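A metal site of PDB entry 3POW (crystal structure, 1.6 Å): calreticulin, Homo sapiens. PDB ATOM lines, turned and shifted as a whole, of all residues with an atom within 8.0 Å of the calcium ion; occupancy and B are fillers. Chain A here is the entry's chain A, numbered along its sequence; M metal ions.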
ATOM      1  N   GLU A  16     -21.782  -2.382  30.109  1.00  0.00           N
ATOM      2  CA  GLU A  16     -22.520  -1.386  29.321  1.00  0.00           C
ATOM      3  C   GLU A  16     -23.612  -2.026  28.526  1.00  0.00           C
ATOM      4  O   GLU A  16     -23.324  -2.851  27.662  1.00  0.00           O
ATOM      5  CB  GLU A  16     -21.586  -0.564  28.407  1.00  0.00           C
ATOM      6  CG  GLU A  16     -22.358   0.428  27.541  1.00  0.00           C
ATOM      7  CD  GLU A  16     -22.909   1.624  28.286  1.00  0.00           C
ATOM      8  OE1 GLU A  16     -22.100   2.536  28.596  1.00  0.00           O
ATOM      9  OE2 GLU A  16     -24.126   1.665  28.566  1.00  0.00           O
ATOM     10  N   GLN A  17     -24.871  -1.621  28.798  1.00  0.00           N
ATOM     11  CA  GLN A  17     -26.043  -2.135  28.124  1.00  0.00           C
ATOM     12  C   GLN A  17     -26.875  -1.064  27.398  1.00  0.00           C
ATOM     13  O   GLN A  17     -27.825  -1.423  26.732  1.00  0.00           O
ATOM     14  CB  GLN A  17     -26.912  -2.953  29.088  1.00  0.00           C
ATOM     15  CG  GLN A  17     -26.143  -4.137  29.688  1.00  0.00           C
ATOM     16  CD  GLN A  17     -27.081  -4.966  30.524  1.00  0.00           C
ATOM     17  OE1 GLN A  17     -27.725  -5.938  30.054  1.00  0.00           O
ATOM     18  NE2 GLN A  17     -27.262  -4.539  31.761  1.00  0.00           N
ATOM     19  N   PHE A  18     -26.509   0.235  27.521  1.00  0.00           N
ATOM     20  CA  PHE A  18     -27.222   1.326  26.830  1.00  0.00           C
ATOM     21  C   PHE A  18     -28.727   1.346  27.181  1.00  0.00           C
ATOM     22  O   PHE A  18     -29.586   1.327  26.286  1.00  0.00           O
ATOM     23  CB  PHE A  18     -26.978   1.266  25.302  1.00  0.00           C
ATOM     24  CG  PHE A  18     -25.526   1.100  24.908  1.00  0.00           C
ATOM     25  CD1 PHE A  18     -24.671   2.201  24.881  1.00  0.00           C
ATOM     26  CD2 PHE A  18     -25.016  -0.152  24.564  1.00  0.00           C
ATOM     27  CE1 PHE A  18     -23.326   2.043  24.545  1.00  0.00           C
ATOM     28  CE2 PHE A  18     -23.677  -0.312  24.234  1.00  0.00           C
ATOM     29  CZ  PHE A  18     -22.835   0.784  24.221  1.00  0.00           C
ATOM     30  N   LEU A  19     -29.030   1.361  28.480  1.00  0.00           N
ATOM     31  CA  LEU A  19     -30.426   1.299  28.967  1.00  0.00           C
ATOM     32  C   LEU A  19     -31.019   2.663  29.311  1.00  0.00           C
ATOM     33  O   LEU A  19     -32.234   2.746  29.593  1.00  0.00           O
ATOM     34  CB  LEU A  19     -30.514   0.380  30.196  1.00  0.00           C
ATOM     35  CG  LEU A  19     -30.069  -1.064  29.982  1.00  0.00           C
ATOM     36  CD1 LEU A  19     -29.898  -1.782  31.314  1.00  0.00           C
ATOM     37  CD2 LEU A  19     -31.037  -1.829  29.080  1.00  0.00           C
ATOM     38  N   ASP A  20     -30.171   3.706  29.345  1.00  0.00           N
ATOM     39  CA  ASP A  20     -30.570   5.056  29.787  1.00  0.00           C
ATOM     40  C   ASP A  20     -30.614   6.126  28.708  1.00  0.00           C
ATOM     41  O   ASP A  20     -30.246   7.283  28.971  1.00  0.00           O
ATOM     42  CB  ASP A  20     -29.712   5.492  30.989  1.00  0.00           C
ATOM     43  CG  ASP A  20     -28.223   5.662  30.699  1.00  0.00           C
ATOM     44  OD1 ASP A  20     -27.761   5.167  29.641  1.00  0.00           O
ATOM     45  OD2 ASP A  20     -27.526   6.241  31.550  1.00  0.00           O
ATOM     46  N   LEU A  42     -27.415   5.287  18.589  1.00  0.00           N
ATOM     47  CA  LEU A  42     -28.070   4.335  19.473  1.00  0.00           C
ATOM     48  C   LEU A  42     -29.308   3.794  18.784  1.00  0.00           C
ATOM     49  O   LEU A  42     -30.232   4.547  18.436  1.00  0.00           O
ATOM     50  CB  LEU A  42     -28.436   4.974  20.830  1.00  0.00           C
ATOM     51  CG  LEU A  42     -29.043   4.026  21.891  1.00  0.00           C
ATOM     52  CD1 LEU A  42     -27.992   3.097  22.475  1.00  0.00           C
ATOM     53  CD2 LEU A  42     -29.710   4.835  22.997  1.00  0.00           C
ATOM     54  N   SER A  43     -29.337   2.448  18.572  1.00  0.00           N
ATOM     55  CA  SER A  43     -30.473   1.829  17.913  1.00  0.00           C
ATOM     56  C   SER A  43     -30.575   0.329  18.195  1.00  0.00           C
ATOM     57  O   SER A  43     -29.568  -0.324  18.484  1.00  0.00           O
ATOM     58  CB  SER A  43     -30.341   1.988  16.391  1.00  0.00           C
ATOM     59  OG  SER A  43     -31.514   1.557  15.715  1.00  0.00           O
ATOM     60  N   SER A  44     -31.806  -0.202  18.073  1.00  0.00           N
ATOM     61  CA  SER A  44     -32.023  -1.649  18.146  1.00  0.00           C
ATOM     62  C   SER A  44     -32.248  -2.219  16.727  1.00  0.00           C
ATOM     63  O   SER A  44     -32.424  -3.433  16.573  1.00  0.00           O
ATOM     64  CB  SER A  44     -33.154  -1.999  19.111  1.00  0.00           C
ATOM     65  OG  SER A  44     -34.297  -1.198  18.853  1.00  0.00           O
ATOM     66  N   ASP A  50     -36.046  -7.311  21.733  1.00  0.00           N
ATOM     67  CA  ASP A  50     -36.825  -6.325  22.489  1.00  0.00           C
ATOM     68  C   ASP A  50     -36.353  -4.940  22.028  1.00  0.00           C
ATOM     69  O   ASP A  50     -35.148  -4.678  22.007  1.00  0.00           O
ATOM     70  CB  ASP A  50     -36.639  -6.519  24.007  1.00  0.00           C
ATOM     71  CG  ASP A  50     -37.418  -5.539  24.876  1.00  0.00           C
ATOM     72  OD1 ASP A  50     -38.517  -5.903  25.350  1.00  0.00           O
ATOM     73  OD2 ASP A  50     -36.985  -4.376  24.990  1.00  0.00           O
ATOM     74  N   GLU A  51     -37.302  -4.067  21.638  1.00  0.00           N
ATOM     75  CA  GLU A  51     -36.978  -2.749  21.082  1.00  0.00           C
ATOM     76  C   GLU A  51     -36.113  -1.877  21.977  1.00  0.00           C
ATOM     77  O   GLU A  51     -35.286  -1.108  21.471  1.00  0.00           O
ATOM     78  CB  GLU A  51     -38.251  -2.007  20.679  1.00  0.00           C
ATOM     79  CG  GLU A  51     -38.006  -0.766  19.822  1.00  0.00           C
ATOM     80  CD  GLU A  51     -39.238  -0.010  19.377  1.00  0.00           C
ATOM     81  OE1 GLU A  51     -40.366  -0.349  19.818  1.00  0.00           O
ATOM     82  OE2 GLU A  51     -39.073   0.935  18.574  1.00  0.00           O
ATOM     83  N   GLU A  52     -36.303  -1.977  23.304  1.00  0.00           N
ATOM     84  CA  GLU A  52     -35.527  -1.184  24.244  1.00  0.00           C
ATOM     85  C   GLU A  52     -34.244  -1.886  24.713  1.00  0.00           C
ATOM     86  O   GLU A  52     -33.178  -1.258  24.721  1.00  0.00           O
ATOM     87  CB  GLU A  52     -36.386  -0.798  25.455  1.00  0.00           C
ATOM     88  CG  GLU A  52     -37.514   0.187  25.143  1.00  0.00           C
ATOM     89  CD  GLU A  52     -37.085   1.497  24.501  1.00  0.00           C
ATOM     90  OE1 GLU A  52     -36.011   2.031  24.900  1.00  0.00           O
ATOM     91  OE2 GLU A  52     -37.793   1.969  23.584  1.00  0.00           O
ATOM     92  N   LYS A  53     -34.352  -3.159  25.164  1.00  0.00           N
ATOM     93  CA  LYS A  53     -33.198  -3.900  25.695  1.00  0.00           C
ATOM     94  C   LYS A  53     -32.113  -4.097  24.635  1.00  0.00           C
ATOM     95  O   LYS A  53     -30.923  -3.984  24.953  1.00  0.00           O
ATOM     96  CB  LYS A  53     -33.646  -5.273  26.256  1.00  0.00           C
ATOM     97  CG  LYS A  53     -34.461  -5.181  27.555  1.00  0.00           C
ATOM     98  CD  LYS A  53     -35.272  -6.449  27.799  1.00  0.00           C
ATOM     99  CE  LYS A  53     -36.226  -6.252  28.956  1.00  0.00           C
ATOM    100  NZ  LYS A  53     -37.423  -7.119  28.857  1.00  0.00           N
ATOM    101  N   ASP A  54     -32.534  -4.283  23.352  1.00  0.00           N
ATOM    102  CA  ASP A  54     -31.604  -4.532  22.255  1.00  0.00           C
ATOM    103  C   ASP A  54     -31.011  -3.309  21.586  1.00  0.00           C
ATOM    104  O   ASP A  54     -30.335  -3.435  20.568  1.00  0.00           O
ATOM    105  CB  ASP A  54     -32.107  -5.622  21.296  1.00  0.00           C
ATOM    106  CG  ASP A  54     -32.185  -6.984  21.990  1.00  0.00           C
ATOM    107  OD1 ASP A  54     -31.168  -7.395  22.626  1.00  0.00           O
ATOM    108  OD2 ASP A  54     -33.268  -7.604  21.954  1.00  0.00           O
ATOM    109  N   LYS A  55     -31.201  -2.110  22.209  1.00  0.00           N
ATOM    110  CA  LYS A  55     -30.522  -0.915  21.714  1.00  0.00           C
ATOM    111  C   LYS A  55     -29.032  -1.061  22.022  1.00  0.00           C
ATOM    112  O   LYS A  55     -28.646  -1.539  23.111  1.00  0.00           O
ATOM    113  CB  LYS A  55     -31.082   0.344  22.399  1.00  0.00           C
ATOM    114  CG  LYS A  55     -32.458   0.722  21.863  1.00  0.00           C
ATOM    115  CD  LYS A  55     -32.971   1.997  22.500  1.00  0.00           C
ATOM    116  CE  LYS A  55     -34.332   2.350  21.941  1.00  0.00           C
ATOM    117  NZ  LYS A  55     -34.895   3.567  22.624  1.00  0.00           N
ATOM    118  N   GLY A  56     -28.199  -0.669  21.055  1.00  0.00           N
ATOM    119  CA  GLY A  56     -26.741  -0.668  21.194  1.00  0.00           C
ATOM    120  C   GLY A  56     -26.114   0.361  20.265  1.00  0.00           C
ATOM    121  O   GLY A  56     -26.842   1.133  19.627  1.00  0.00           O
ATOM    122  N   LEU A  57     -24.767   0.375  20.187  1.00  0.00           N
ATOM    123  CA  LEU A  57     -24.065   1.318  19.302  1.00  0.00           C
ATOM    124  C   LEU A  57     -24.052   0.762  17.888  1.00  0.00           C
ATOM    125  O   LEU A  57     -23.560  -0.347  17.673  1.00  0.00           O
ATOM    126  CB  LEU A  57     -22.604   1.509  19.764  1.00  0.00           C
ATOM    127  CG  LEU A  57     -22.408   2.158  21.111  1.00  0.00           C
ATOM    128  CD1 LEU A  57     -20.940   2.061  21.542  1.00  0.00           C
ATOM    129  CD2 LEU A  57     -22.940   3.580  21.118  1.00  0.00           C
ATOM    130  N   THR A  87     -21.692  -8.362  22.560  1.00  0.00           N
ATOM    131  CA  THR A  87     -22.455  -8.934  21.448  1.00  0.00           C
ATOM    132  C   THR A  87     -22.166  -8.103  20.183  1.00  0.00           C
ATOM    133  O   THR A  87     -21.956  -6.875  20.260  1.00  0.00           O
ATOM    134  CB  THR A  87     -23.974  -8.997  21.730  1.00  0.00           C
ATOM    135  OG1 THR A  87     -24.478  -7.685  21.958  1.00  0.00           O
ATOM    136  CG2 THR A  87     -24.347  -9.920  22.925  1.00  0.00           C
ATOM    137  N   ILE A 223     -24.441  -3.544  15.071  1.00  0.00           N
ATOM    138  CA  ILE A 223     -24.795  -3.108  16.416  1.00  0.00           C
ATOM    139  C   ILE A 223     -23.967  -3.857  17.472  1.00  0.00           C
ATOM    140  O   ILE A 223     -23.910  -5.097  17.450  1.00  0.00           O
ATOM    141  CB  ILE A 223     -26.315  -3.246  16.715  1.00  0.00           C
ATOM    142  CG1 ILE A 223     -27.152  -2.541  15.635  1.00  0.00           C
ATOM    143  CG2 ILE A 223     -26.651  -2.769  18.133  1.00  0.00           C
ATOM    144  CD1 ILE A 223     -28.678  -2.653  15.836  1.00  0.00           C
ATOM    145  N   PHE A 224     -23.377  -3.105  18.419  1.00  0.00           N
ATOM    146  CA  PHE A 224     -22.613  -3.626  19.545  1.00  0.00           C
ATOM    147  C   PHE A 224     -23.402  -3.392  20.846  1.00  0.00           C
ATOM    148  O   PHE A 224     -23.935  -2.294  21.047  1.00  0.00           O
ATOM    149  CB  PHE A 224     -21.254  -2.891  19.643  1.00  0.00           C
ATOM    150  CG  PHE A 224     -20.387  -3.066  18.409  1.00  0.00           C
ATOM    151  CD1 PHE A 224     -19.553  -4.168  18.284  1.00  0.00           C
ATOM    152  CD2 PHE A 224     -20.451  -2.159  17.357  1.00  0.00           C
ATOM    153  CE1 PHE A 224     -18.772  -4.352  17.135  1.00  0.00           C
ATOM    154  CE2 PHE A 224     -19.650  -2.336  16.201  1.00  0.00           C
ATOM    155  CZ  PHE A 224     -18.826  -3.432  16.098  1.00  0.00           C
ATOM    156  N   ASP A 225     -23.459  -4.385  21.724  1.00  0.00           N
ATOM    157  CA  ASP A 225     -24.209  -4.262  22.982  1.00  0.00           C
ATOM    158  C   ASP A 225     -23.620  -5.181  24.052  1.00  0.00           C
ATOM    159  O   ASP A 225     -22.709  -5.973  23.788  1.00  0.00           O
ATOM    160  CB  ASP A 225     -25.682  -4.685  22.705  1.00  0.00           C
ATOM    161  CG  ASP A 225     -26.764  -4.147  23.650  1.00  0.00           C
ATOM    162  OD1 ASP A 225     -26.417  -3.444  24.630  1.00  0.00           O
ATOM    163  OD2 ASP A 225     -27.948  -4.472  23.426  1.00  0.00           O
ATOM    164  N   ASN A 226     -24.126  -5.042  25.295  1.00  0.00           N
ATOM    165  CA  ASN A 226     -23.885  -5.926  26.426  1.00  0.00           C
ATOM    166  C   ASN A 226     -22.404  -6.196  26.684  1.00  0.00           C
ATOM    167  O   ASN A 226     -21.962  -7.348  26.792  1.00  0.00           O
ATOM    168  CB  ASN A 226     -24.715  -7.215  26.229  1.00  0.00           C
ATOM    169  CG  ASN A 226     -26.190  -6.922  26.142  1.00  0.00           C
ATOM    170  OD1 ASN A 226     -26.890  -7.328  25.174  1.00  0.00           O
ATOM    171  ND2 ASN A 226     -26.698  -6.207  27.142  1.00  0.00           N
ATOM    172  N   PHE A 227     -21.642  -5.108  26.792  1.00  0.00           N
ATOM    173  CA  PHE A 227     -20.223  -5.212  27.117  1.00  0.00           C
ATOM    174  C   PHE A 227     -20.025  -5.608  28.580  1.00  0.00           C
ATOM    175  O   PHE A 227     -20.720  -5.115  29.456  1.00  0.00           O
ATOM    176  CB  PHE A 227     -19.523  -3.861  26.879  1.00  0.00           C
ATOM    177  CG  PHE A 227     -19.466  -3.406  25.438  1.00  0.00           C
ATOM    178  CD1 PHE A 227     -18.350  -3.674  24.658  1.00  0.00           C
ATOM    179  CD2 PHE A 227     -20.479  -2.616  24.903  1.00  0.00           C
ATOM    180  CE1 PHE A 227     -18.305  -3.260  23.322  1.00  0.00           C
ATOM    181  CE2 PHE A 227     -20.420  -2.198  23.566  1.00  0.00           C
ATOM    182  CZ  PHE A 227     -19.330  -2.504  22.791  1.00  0.00           C
ATOM    183  N   THR A 243     -28.472 -11.912  28.460  1.00  0.00           N
ATOM    184  CA  THR A 243     -28.432 -10.853  27.445  1.00  0.00           C
ATOM    185  C   THR A 243     -28.632 -11.460  26.065  1.00  0.00           C
ATOM    186  O   THR A 243     -29.773 -11.509  25.588  1.00  0.00           O
ATOM    187  CB  THR A 243     -27.162 -10.012  27.620  1.00  0.00           C
ATOM    188  OG1 THR A 243     -25.990 -10.877  27.513  1.00  0.00           O
ATOM    189  CG2 THR A 243     -27.155  -9.259  28.959  1.00  0.00           C
ATOM    190  N   THR A 247     -32.113 -12.327  23.912  1.00  0.00           N
ATOM    191  CA  THR A 247     -32.336 -11.689  22.619  1.00  0.00           C
ATOM    192  C   THR A 247     -32.666 -12.712  21.506  1.00  0.00           C
ATOM    193  O   THR A 247     -33.495 -12.442  20.634  1.00  0.00           O
ATOM    194  CB  THR A 247     -31.027 -10.969  22.206  1.00  0.00           C
ATOM    195  OG1 THR A 247     -30.696  -9.968  23.168  1.00  0.00           O
ATOM    196  CG2 THR A 247     -31.048 -10.390  20.773  1.00  0.00           C
HETATM  197 CA    CA M   1     -28.818  -2.817  25.099  1.00  0.00          CA
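The calcium ion is bound by O of Gln 17, O of Lys 55, O of Lys 53, OD2 of Asp 225 and OD1 of Asp 225.
The side-chain carboxylate (OE1) of Glu 52 lies within salt-bridge range of the side-chain amino group (NZ) of Lys 55.
The backbone carbonyl oxygen of Asp 225 is in hydrogen-bond range of the backbone NH of Thr 87.
OE1 of Gln 17 lies within hydrogen-bond range of ND2 of Asn 226 (3.1 Å).
NZ of Lys 53 lies within salt-bridge range of OD1 of Asp 50 (3.9 Å).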
